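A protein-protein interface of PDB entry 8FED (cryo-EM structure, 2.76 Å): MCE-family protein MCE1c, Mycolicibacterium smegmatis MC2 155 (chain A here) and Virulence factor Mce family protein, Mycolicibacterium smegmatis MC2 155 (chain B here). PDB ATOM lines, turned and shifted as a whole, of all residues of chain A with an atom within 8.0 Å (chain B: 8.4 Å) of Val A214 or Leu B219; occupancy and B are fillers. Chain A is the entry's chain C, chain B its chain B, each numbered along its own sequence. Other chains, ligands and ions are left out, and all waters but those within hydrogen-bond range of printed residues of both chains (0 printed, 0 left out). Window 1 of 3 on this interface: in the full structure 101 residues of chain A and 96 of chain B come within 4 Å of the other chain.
OD2 of Asp B216 is in salt-bridge range of NH2 of Arg A210.
The side-chain carboxylate (OE2) of Glu B223 sits close to the side-chain amide oxygen (OE1) of Gln A216 (3.0 Å).
The backbone carbonyl oxygen of Val B220 sits at hydrogen-bond distance from the side-chain hydroxyl of Thr B224 (2.9 Å).
OE1 of Glu B223 is in hydrogen-bond range of OG1 of Thr B224, 3.5 Å away.
The backbone carbonyl oxygen (O) of Gln A216 lies close to the side-chain amide oxygen (OD1) of Asn A220.
CG2 of Val A206 touches NE2 of Gln B212, 3.6 Å away.
Val A206 touches Phe B215 (CG1 to CD2, 3.6 Å).
CG1 of Val A206 touches OD1 of Asp B216 (3.4 Å).
Val B220 touches Arg A210.
Val A214 touches Leu B219 (CG2 to CD1, 3.96 Å).
Leu A217 touches Leu B219.
CD1 of Leu A217 touches CB of Phe B222, at 3.6 Å.
CG2 of Ile B226 touches O of Leu A217, 3.5 Å away.
Asn A220 touches Ile B226.
Ile B226 touches Ala A221.
Printed residues of chain B within 4 Å of Gln A213: Glu B223 (3.2 Å).
Of chain B, only Leu B219 comes within 4 Å of Val A214.
Printed residues of chain B within 4 Å of Gln A216: Glu B223 (3.0 Å).
Of the printed residues of chain B, Leu A217 touches Leu B219, Phe B222, Glu B223 and Ile B226.
Of the printed residues of chain B, Asn A220 touches Ile B226.
No residue of chain A comes within 4 Å of Thr B218.
Leu B219 touches two residues of chain A.
Of the printed residues of chain A, Ile B226 touches Leu A217 (3.5 Å), Asn A220 (3.6 Å) and Ala A221 (3.3 Å).
The nearest residue of chain B that does not touch Val A214 is Glu B223 (5.2 Å).
The nearest residue of chain A that does not touch Leu B219 is Arg A210 (4.1 Å).
Of the 17 printed residues of chain A, 8 touch a printed residue of chain B.
Of the 15 printed residues of chain B, 8 touch a printed residue of chain A.
Among the printed residues, 14 pairs touch across the chains.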
ATOM      1  N   VAL A 203     -32.761  13.937 -11.896  1.00  0.00           N
ATOM      2  CA  VAL A 203     -32.635  14.478 -13.249  1.00  0.00           C
ATOM      3  C   VAL A 203     -31.420  15.396 -13.361  1.00  0.00           C
ATOM      4  O   VAL A 203     -30.659  15.326 -14.336  1.00  0.00           O
ATOM      5  CB  VAL A 203     -33.933  15.197 -13.658  1.00  0.00           C
ATOM      6  CG1 VAL A 203     -33.770  15.859 -15.014  1.00  0.00           C
ATOM      7  CG2 VAL A 203     -35.086  14.212 -13.693  1.00  0.00           C
ATOM      8  N   VAL A 206     -28.249  13.429 -13.469  1.00  0.00           N
ATOM      9  CA  VAL A 206     -28.037  12.877 -14.806  1.00  0.00           C
ATOM     10  C   VAL A 206     -27.503  13.948 -15.750  1.00  0.00           C
ATOM     11  O   VAL A 206     -26.581  13.699 -16.538  1.00  0.00           O
ATOM     12  CB  VAL A 206     -29.334  12.244 -15.340  1.00  0.00           C
ATOM     13  CG1 VAL A 206     -29.164  11.834 -16.791  1.00  0.00           C
ATOM     14  CG2 VAL A 206     -29.708  11.039 -14.499  1.00  0.00           C
ATOM     15  N   LEU A 207     -28.069  15.156 -15.686  1.00  0.00           N
ATOM     16  CA  LEU A 207     -27.615  16.240 -16.554  1.00  0.00           C
ATOM     17  C   LEU A 207     -26.175  16.640 -16.246  1.00  0.00           C
ATOM     18  O   LEU A 207     -25.357  16.809 -17.157  1.00  0.00           O
ATOM     19  CB  LEU A 207     -28.540  17.450 -16.422  1.00  0.00           C
ATOM     20  CG  LEU A 207     -29.877  17.381 -17.159  1.00  0.00           C
ATOM     21  CD1 LEU A 207     -30.672  18.654 -16.929  1.00  0.00           C
ATOM     22  CD2 LEU A 207     -29.652  17.150 -18.642  1.00  0.00           C
ATOM     23  N   GLY A 208     -25.850  16.799 -14.962  1.00  0.00           N
ATOM     24  CA  GLY A 208     -24.521  17.253 -14.587  1.00  0.00           C
ATOM     25  C   GLY A 208     -23.439  16.238 -14.899  1.00  0.00           C
ATOM     26  O   GLY A 208     -22.336  16.604 -15.314  1.00  0.00           O
ATOM     27  N   ASP A 209     -23.727  14.950 -14.685  1.00  0.00           N
ATOM     28  CA  ASP A 209     -22.744  13.920 -15.001  1.00  0.00           C
ATOM     29  C   ASP A 209     -22.427  13.860 -16.490  1.00  0.00           C
ATOM     30  O   ASP A 209     -21.358  13.370 -16.867  1.00  0.00           O
ATOM     31  CB  ASP A 209     -23.230  12.553 -14.518  1.00  0.00           C
ATOM     32  CG  ASP A 209     -23.344  12.476 -13.010  1.00  0.00           C
ATOM     33  OD1 ASP A 209     -23.071  13.493 -12.341  1.00  0.00           O
ATOM     34  OD2 ASP A 209     -23.704  11.398 -12.494  1.00  0.00           O
ATOM     35  N   ARG A 210     -23.334  14.344 -17.343  1.00  0.00           N
ATOM     36  CA  ARG A 210     -23.143  14.334 -18.788  1.00  0.00           C
ATOM     37  C   ARG A 210     -23.067  15.742 -19.372  1.00  0.00           C
ATOM     38  O   ARG A 210     -23.311  15.923 -20.568  1.00  0.00           O
ATOM     39  CB  ARG A 210     -24.264  13.545 -19.466  1.00  0.00           C
ATOM     40  CG  ARG A 210     -24.474  12.154 -18.896  1.00  0.00           C
ATOM     41  CD  ARG A 210     -23.200  11.336 -18.966  1.00  0.00           C
ATOM     42  NE  ARG A 210     -23.404   9.972 -18.494  1.00  0.00           N
ATOM     43  CZ  ARG A 210     -22.463   9.038 -18.478  1.00  0.00           C
ATOM     44  NH1 ARG A 210     -21.235   9.287 -18.904  1.00  0.00           N
ATOM     45  NH2 ARG A 210     -22.762   7.824 -18.025  1.00  0.00           N
ATOM     46  N   SER A 211     -22.737  16.742 -18.550  1.00  0.00           N
ATOM     47  CA  SER A 211     -22.735  18.126 -19.019  1.00  0.00           C
ATOM     48  C   SER A 211     -21.675  18.364 -20.089  1.00  0.00           C
ATOM     49  O   SER A 211     -21.919  19.094 -21.058  1.00  0.00           O
ATOM     50  CB  SER A 211     -22.520  19.078 -17.851  1.00  0.00           C
ATOM     51  OG  SER A 211     -22.481  20.410 -18.320  1.00  0.00           O
ATOM     52  N   THR A 212     -20.485  17.785 -19.916  1.00  0.00           N
ATOM     53  CA  THR A 212     -19.451  17.910 -20.939  1.00  0.00           C
ATOM     54  C   THR A 212     -19.922  17.312 -22.255  1.00  0.00           C
ATOM     55  O   THR A 212     -19.717  17.899 -23.326  1.00  0.00           O
ATOM     56  CB  THR A 212     -18.162  17.231 -20.468  1.00  0.00           C
ATOM     57  OG1 THR A 212     -17.683  17.882 -19.285  1.00  0.00           O
ATOM     58  CG2 THR A 212     -17.092  17.303 -21.545  1.00  0.00           C
ATOM     59  N   GLN A 213     -20.577  16.150 -22.187  1.00  0.00           N
ATOM     60  CA  GLN A 213     -21.129  15.531 -23.386  1.00  0.00           C
ATOM     61  C   GLN A 213     -22.199  16.411 -24.017  1.00  0.00           C
ATOM     62  O   GLN A 213     -22.269  16.523 -25.242  1.00  0.00           O
ATOM     63  CB  GLN A 213     -21.694  14.150 -23.057  1.00  0.00           C
ATOM     64  CG  GLN A 213     -20.645  13.072 -22.803  1.00  0.00           C
ATOM     65  CD  GLN A 213     -19.977  13.191 -21.446  1.00  0.00           C
ATOM     66  OE1 GLN A 213     -20.334  14.044 -20.634  1.00  0.00           O
ATOM     67  NE2 GLN A 213     -19.001  12.327 -21.194  1.00  0.00           N
ATOM     68  N   VAL A 214     -23.044  17.044 -23.199  1.00  0.00           N
ATOM     69  CA  VAL A 214     -24.092  17.914 -23.733  1.00  0.00           C
ATOM     70  C   VAL A 214     -23.481  19.105 -24.464  1.00  0.00           C
ATOM     71  O   VAL A 214     -23.898  19.453 -25.577  1.00  0.00           O
ATOM     72  CB  VAL A 214     -25.039  18.367 -22.608  1.00  0.00           C
ATOM     73  CG1 VAL A 214     -25.943  19.488 -23.089  1.00  0.00           C
ATOM     74  CG2 VAL A 214     -25.874  17.199 -22.120  1.00  0.00           C
ATOM     75  N   ASN A 215     -22.486  19.750 -23.848  1.00  0.00           N
ATOM     76  CA  ASN A 215     -21.853  20.907 -24.477  1.00  0.00           C
ATOM     77  C   ASN A 215     -21.153  20.518 -25.773  1.00  0.00           C
ATOM     78  O   ASN A 215     -21.277  21.213 -26.793  1.00  0.00           O
ATOM     79  CB  ASN A 215     -20.864  21.553 -23.507  1.00  0.00           C
ATOM     80  CG  ASN A 215     -20.263  22.830 -24.052  1.00  0.00           C
ATOM     81  OD1 ASN A 215     -20.853  23.493 -24.905  1.00  0.00           O
ATOM     82  ND2 ASN A 215     -19.083  23.186 -23.559  1.00  0.00           N
ATOM     83  N   GLN A 216     -20.411  19.408 -25.748  1.00  0.00           N
ATOM     84  CA  GLN A 216     -19.727  18.942 -26.948  1.00  0.00           C
ATOM     85  C   GLN A 216     -20.727  18.581 -28.038  1.00  0.00           C
ATOM     86  O   GLN A 216     -20.508  18.883 -29.216  1.00  0.00           O
ATOM     87  CB  GLN A 216     -18.835  17.751 -26.602  1.00  0.00           C
ATOM     88  CG  GLN A 216     -17.840  17.372 -27.676  1.00  0.00           C
ATOM     89  CD  GLN A 216     -16.828  16.357 -27.188  1.00  0.00           C
ATOM     90  OE1 GLN A 216     -16.934  15.845 -26.074  1.00  0.00           O
ATOM     91  NE2 GLN A 216     -15.838  16.061 -28.021  1.00  0.00           N
ATOM     92  N   LEU A 217     -21.837  17.945 -27.657  1.00  0.00           N
ATOM     93  CA  LEU A 217     -22.891  17.605 -28.605  1.00  0.00           C
ATOM     94  C   LEU A 217     -23.447  18.857 -29.268  1.00  0.00           C
ATOM     95  O   LEU A 217     -23.607  18.902 -30.490  1.00  0.00           O
ATOM     96  CB  LEU A 217     -23.998  16.839 -27.874  1.00  0.00           C
ATOM     97  CG  LEU A 217     -25.094  16.014 -28.556  1.00  0.00           C
ATOM     98  CD1 LEU A 217     -25.841  15.248 -27.483  1.00  0.00           C
ATOM     99  CD2 LEU A 217     -26.078  16.844 -29.369  1.00  0.00           C
ATOM    100  N   LEU A 218     -23.749  19.883 -28.471  1.00  0.00           N
ATOM    101  CA  LEU A 218     -24.336  21.096 -29.033  1.00  0.00           C
ATOM    102  C   LEU A 218     -23.367  21.807 -29.971  1.00  0.00           C
ATOM    103  O   LEU A 218     -23.761  22.239 -31.062  1.00  0.00           O
ATOM    104  CB  LEU A 218     -24.795  22.029 -27.913  1.00  0.00           C
ATOM    105  CG  LEU A 218     -25.975  21.510 -27.090  1.00  0.00           C
ATOM    106  CD1 LEU A 218     -26.498  22.575 -26.145  1.00  0.00           C
ATOM    107  CD2 LEU A 218     -27.081  21.020 -28.004  1.00  0.00           C
ATOM    108  N   VAL A 219     -22.094  21.927 -29.578  1.00  0.00           N
ATOM    109  CA  VAL A 219     -21.154  22.650 -30.433  1.00  0.00           C
ATOM    110  C   VAL A 219     -20.859  21.859 -31.707  1.00  0.00           C
ATOM    111  O   VAL A 219     -20.771  22.435 -32.801  1.00  0.00           O
ATOM    112  CB  VAL A 219     -19.873  23.025 -29.659  1.00  0.00           C
ATOM    113  CG1 VAL A 219     -20.217  23.929 -28.484  1.00  0.00           C
ATOM    114  CG2 VAL A 219     -19.113  21.799 -29.182  1.00  0.00           C
ATOM    115  N   ASN A 220     -20.720  20.532 -31.600  1.00  0.00           N
ATOM    116  CA  ASN A 220     -20.505  19.725 -32.794  1.00  0.00           C
ATOM    117  C   ASN A 220     -21.726  19.740 -33.703  1.00  0.00           C
ATOM    118  O   ASN A 220     -21.581  19.707 -34.927  1.00  0.00           O
ATOM    119  CB  ASN A 220     -20.142  18.290 -32.413  1.00  0.00           C
ATOM    120  CG  ASN A 220     -18.806  18.192 -31.708  1.00  0.00           C
ATOM    121  OD1 ASN A 220     -18.631  17.380 -30.801  1.00  0.00           O
ATOM    122  ND2 ASN A 220     -17.859  19.031 -32.109  1.00  0.00           N
ATOM    123  N   ALA A 221     -22.932  19.787 -33.130  1.00  0.00           N
ATOM    124  CA  ALA A 221     -24.137  19.886 -33.944  1.00  0.00           C
ATOM    125  C   ALA A 221     -24.195  21.219 -34.672  1.00  0.00           C
ATOM    126  O   ALA A 221     -24.599  21.274 -35.839  1.00  0.00           O
ATOM    127  CB  ALA A 221     -25.377  19.693 -33.074  1.00  0.00           C
ATOM    128  N   GLN B 212     -34.697   6.888 -16.368  1.00  0.00           N
ATOM    129  CA  GLN B 212     -33.454   7.567 -16.009  1.00  0.00           C
ATOM    130  C   GLN B 212     -32.243   6.924 -16.674  1.00  0.00           C
ATOM    131  O   GLN B 212     -31.346   7.625 -17.154  1.00  0.00           O
ATOM    132  CB  GLN B 212     -33.283   7.575 -14.491  1.00  0.00           C
ATOM    133  CG  GLN B 212     -32.000   8.219 -14.006  1.00  0.00           C
ATOM    134  CD  GLN B 212     -31.869   8.184 -12.497  1.00  0.00           C
ATOM    135  OE1 GLN B 212     -32.752   7.687 -11.797  1.00  0.00           O
ATOM    136  NE2 GLN B 212     -30.764   8.714 -11.986  1.00  0.00           N
ATOM    137  N   LYS B 213     -32.196   5.589 -16.706  1.00  0.00           N
ATOM    138  CA  LYS B 213     -31.078   4.897 -17.339  1.00  0.00           C
ATOM    139  C   LYS B 213     -31.003   5.221 -18.827  1.00  0.00           C
ATOM    140  O   LYS B 213     -29.932   5.551 -19.354  1.00  0.00           O
ATOM    141  CB  LYS B 213     -31.210   3.390 -17.120  1.00  0.00           C
ATOM    142  CG  LYS B 213     -29.968   2.592 -17.469  1.00  0.00           C
ATOM    143  CD  LYS B 213     -28.844   2.877 -16.486  1.00  0.00           C
ATOM    144  CE  LYS B 213     -27.718   1.866 -16.623  1.00  0.00           C
ATOM    145  NZ  LYS B 213     -27.194   1.797 -18.014  1.00  0.00           N
ATOM    146  N   GLN B 214     -32.142   5.147 -19.520  1.00  0.00           N
ATOM    147  CA  GLN B 214     -32.158   5.424 -20.952  1.00  0.00           C
ATOM    148  C   GLN B 214     -31.892   6.897 -21.231  1.00  0.00           C
ATOM    149  O   GLN B 214     -31.201   7.233 -22.197  1.00  0.00           O
ATOM    150  CB  GLN B 214     -33.494   4.990 -21.554  1.00  0.00           C
ATOM    151  CG  GLN B 214     -34.022   3.668 -21.015  1.00  0.00           C
ATOM    152  CD  GLN B 214     -33.103   2.496 -21.306  1.00  0.00           C
ATOM    153  OE1 GLN B 214     -32.361   2.500 -22.289  1.00  0.00           O
ATOM    154  NE2 GLN B 214     -33.149   1.483 -20.450  1.00  0.00           N
ATOM    155  N   PHE B 215     -32.439   7.788 -20.400  1.00  0.00           N
ATOM    156  CA  PHE B 215     -32.192   9.216 -20.575  1.00  0.00           C
ATOM    157  C   PHE B 215     -30.726   9.559 -20.342  1.00  0.00           C
ATOM    158  O   PHE B 215     -30.206  10.498 -20.953  1.00  0.00           O
ATOM    159  CB  PHE B 215     -33.091  10.019 -19.637  1.00  0.00           C
ATOM    160  CG  PHE B 215     -32.801  11.491 -19.626  1.00  0.00           C
ATOM    161  CD1 PHE B 215     -33.065  12.270 -20.738  1.00  0.00           C
ATOM    162  CD2 PHE B 215     -32.284  12.097 -18.497  1.00  0.00           C
ATOM    163  CE1 PHE B 215     -32.804  13.628 -20.727  1.00  0.00           C
ATOM    164  CE2 PHE B 215     -32.021  13.454 -18.480  1.00  0.00           C
ATOM    165  CZ  PHE B 215     -32.284  14.219 -19.596  1.00  0.00           C
ATOM    166  N   ASP B 216     -30.052   8.822 -19.458  1.00  0.00           N
ATOM    167  CA  ASP B 216     -28.627   9.041 -19.247  1.00  0.00           C
ATOM    168  C   ASP B 216     -27.807   8.496 -20.410  1.00  0.00           C
ATOM    169  O   ASP B 216     -26.852   9.141 -20.857  1.00  0.00           O
ATOM    170  CB  ASP B 216     -28.189   8.393 -17.933  1.00  0.00           C
ATOM    171  CG  ASP B 216     -26.751   8.707 -17.578  1.00  0.00           C
ATOM    172  OD1 ASP B 216     -26.488   9.829 -17.099  1.00  0.00           O
ATOM    173  OD2 ASP B 216     -25.885   7.830 -17.777  1.00  0.00           O
ATOM    174  N   GLU B 217     -28.163   7.311 -20.913  1.00  0.00           N
ATOM    175  CA  GLU B 217     -27.398   6.712 -22.004  1.00  0.00           C
ATOM    176  C   GLU B 217     -27.586   7.457 -23.320  1.00  0.00           C
ATOM    177  O   GLU B 217     -26.656   7.508 -24.138  1.00  0.00           O
ATOM    178  CB  GLU B 217     -27.786   5.244 -22.180  1.00  0.00           C
ATOM    179  CG  GLU B 217     -27.444   4.356 -20.999  1.00  0.00           C
ATOM    180  CD  GLU B 217     -27.848   2.913 -21.224  1.00  0.00           C
ATOM    181  OE1 GLU B 217     -28.185   2.562 -22.375  1.00  0.00           O
ATOM    182  OE2 GLU B 217     -27.832   2.129 -20.253  1.00  0.00           O
ATOM    183  N   THR B 218     -28.773   8.028 -23.553  1.00  0.00           N
ATOM    184  CA  THR B 218     -29.038   8.654 -24.843  1.00  0.00           C
ATOM    185  C   THR B 218     -28.219   9.922 -25.038  1.00  0.00           C
ATOM    186  O   THR B 218     -27.851  10.237 -26.171  1.00  0.00           O
ATOM    187  CB  THR B 218     -30.534   8.940 -25.013  1.00  0.00           C
ATOM    188  OG1 THR B 218     -30.774   9.438 -26.335  1.00  0.00           O
ATOM    189  CG2 THR B 218     -31.027   9.964 -24.010  1.00  0.00           C
ATOM    190  N   LEU B 219     -27.912  10.653 -23.963  1.00  0.00           N
ATOM    191  CA  LEU B 219     -27.053  11.827 -24.096  1.00  0.00           C
ATOM    192  C   LEU B 219     -25.662  11.431 -24.575  1.00  0.00           C
ATOM    193  O   LEU B 219     -25.109  12.050 -25.491  1.00  0.00           O
ATOM    194  CB  LEU B 219     -26.974  12.578 -22.766  1.00  0.00           C
ATOM    195  CG  LEU B 219     -28.252  13.282 -22.314  1.00  0.00           C
ATOM    196  CD1 LEU B 219     -28.015  14.047 -21.024  1.00  0.00           C
ATOM    197  CD2 LEU B 219     -28.759  14.209 -23.403  1.00  0.00           C
ATOM    198  N   VAL B 220     -25.090  10.382 -23.977  1.00  0.00           N
ATOM    199  CA  VAL B 220     -23.769   9.912 -24.385  1.00  0.00           C
ATOM    200  C   VAL B 220     -23.799   9.412 -25.823  1.00  0.00           C
ATOM    201  O   VAL B 220     -22.906   9.724 -26.622  1.00  0.00           O
ATOM    202  CB  VAL B 220     -23.271   8.819 -23.421  1.00  0.00           C
ATOM    203  CG1 VAL B 220     -21.901   8.318 -23.847  1.00  0.00           C
ATOM    204  CG2 VAL B 220     -23.234   9.345 -22.002  1.00  0.00           C
ATOM    205  N   ASN B 221     -24.820   8.625 -26.173  1.00  0.00           N
ATOM    206  CA  ASN B 221     -24.894   8.085 -27.528  1.00  0.00           C
ATOM    207  C   ASN B 221     -25.077   9.193 -28.559  1.00  0.00           C
ATOM    208  O   ASN B 221     -24.456   9.166 -29.629  1.00  0.00           O
ATOM    209  CB  ASN B 221     -26.024   7.060 -27.628  1.00  0.00           C
ATOM    210  CG  ASN B 221     -25.735   5.802 -26.838  1.00  0.00           C
ATOM    211  OD1 ASN B 221     -26.523   5.394 -25.986  1.00  0.00           O
ATOM    212  ND2 ASN B 221     -24.596   5.179 -27.116  1.00  0.00           N
ATOM    213  N   PHE B 222     -25.924  10.177 -28.256  1.00  0.00           N
ATOM    214  CA  PHE B 222     -26.136  11.290 -29.171  1.00  0.00           C
ATOM    215  C   PHE B 222     -24.871  12.120 -29.325  1.00  0.00           C
ATOM    216  O   PHE B 222     -24.546  12.557 -30.432  1.00  0.00           O
ATOM    217  CB  PHE B 222     -27.296  12.154 -28.679  1.00  0.00           C
ATOM    218  CG  PHE B 222     -28.054  12.838 -29.780  1.00  0.00           C
ATOM    219  CD1 PHE B 222     -27.708  12.642 -31.106  1.00  0.00           C
ATOM    220  CD2 PHE B 222     -29.114  13.678 -29.487  1.00  0.00           C
ATOM    221  CE1 PHE B 222     -28.405  13.269 -32.118  1.00  0.00           C
ATOM    222  CE2 PHE B 222     -29.814  14.308 -30.495  1.00  0.00           C
ATOM    223  CZ  PHE B 222     -29.459  14.104 -31.811  1.00  0.00           C
ATOM    224  N   GLU B 223     -24.144  12.351 -28.226  1.00  0.00           N
ATOM    225  CA  GLU B 223     -22.882  13.074 -28.319  1.00  0.00           C
ATOM    226  C   GLU B 223     -21.886  12.320 -29.187  1.00  0.00           C
ATOM    227  O   GLU B 223     -21.192  12.924 -30.012  1.00  0.00           O
ATOM    228  CB  GLU B 223     -22.311  13.318 -26.919  1.00  0.00           C
ATOM    229  CG  GLU B 223     -20.982  14.070 -26.883  1.00  0.00           C
ATOM    230  CD  GLU B 223     -19.772  13.158 -26.970  1.00  0.00           C
ATOM    231  OE1 GLU B 223     -19.936  11.929 -26.824  1.00  0.00           O
ATOM    232  OE2 GLU B 223     -18.654  13.671 -27.188  1.00  0.00           O
ATOM    233  N   THR B 224     -21.803  10.998 -29.016  1.00  0.00           N
ATOM    234  CA  THR B 224     -20.890  10.204 -29.833  1.00  0.00           C
ATOM    235  C   THR B 224     -21.264  10.281 -31.309  1.00  0.00           C
ATOM    236  O   THR B 224     -20.394  10.462 -32.169  1.00  0.00           O
ATOM    237  CB  THR B 224     -20.889   8.752 -29.355  1.00  0.00           C
ATOM    238  OG1 THR B 224     -20.510   8.704 -27.974  1.00  0.00           O
ATOM    239  CG2 THR B 224     -19.909   7.924 -30.167  1.00  0.00           C
ATOM    240  N   LEU B 225     -22.560  10.163 -31.616  1.00  0.00           N
ATOM    241  CA  LEU B 225     -23.009  10.235 -33.004  1.00  0.00           C
ATOM    242  C   LEU B 225     -22.721  11.603 -33.614  1.00  0.00           C
ATOM    243  O   LEU B 225     -22.234  11.698 -34.748  1.00  0.00           O
ATOM    244  CB  LEU B 225     -24.502   9.918 -33.082  1.00  0.00           C
ATOM    245  CG  LEU B 225     -25.221  10.253 -34.390  1.00  0.00           C
ATOM    246  CD1 LEU B 225     -24.700   9.401 -35.532  1.00  0.00           C
ATOM    247  CD2 LEU B 225     -26.721  10.084 -34.229  1.00  0.00           C
ATOM    248  N   ILE B 226     -23.013  12.673 -32.872  1.00  0.00           N
ATOM    249  CA  ILE B 226     -22.824  14.018 -33.399  1.00  0.00           C
ATOM    250  C   ILE B 226     -21.342  14.316 -33.590  1.00  0.00           C
ATOM    251  O   ILE B 226     -20.950  14.952 -34.572  1.00  0.00           O
ATOM    252  CB  ILE B 226     -23.513  15.051 -32.490  1.00  0.00           C
ATOM    253  CG1 ILE B 226     -25.028  14.856 -32.528  1.00  0.00           C
ATOM    254  CG2 ILE B 226     -23.198  16.457 -32.933  1.00  0.00           C
ATOM    255  CD1 ILE B 226     -25.622  15.000 -33.910  1.00  0.00           C
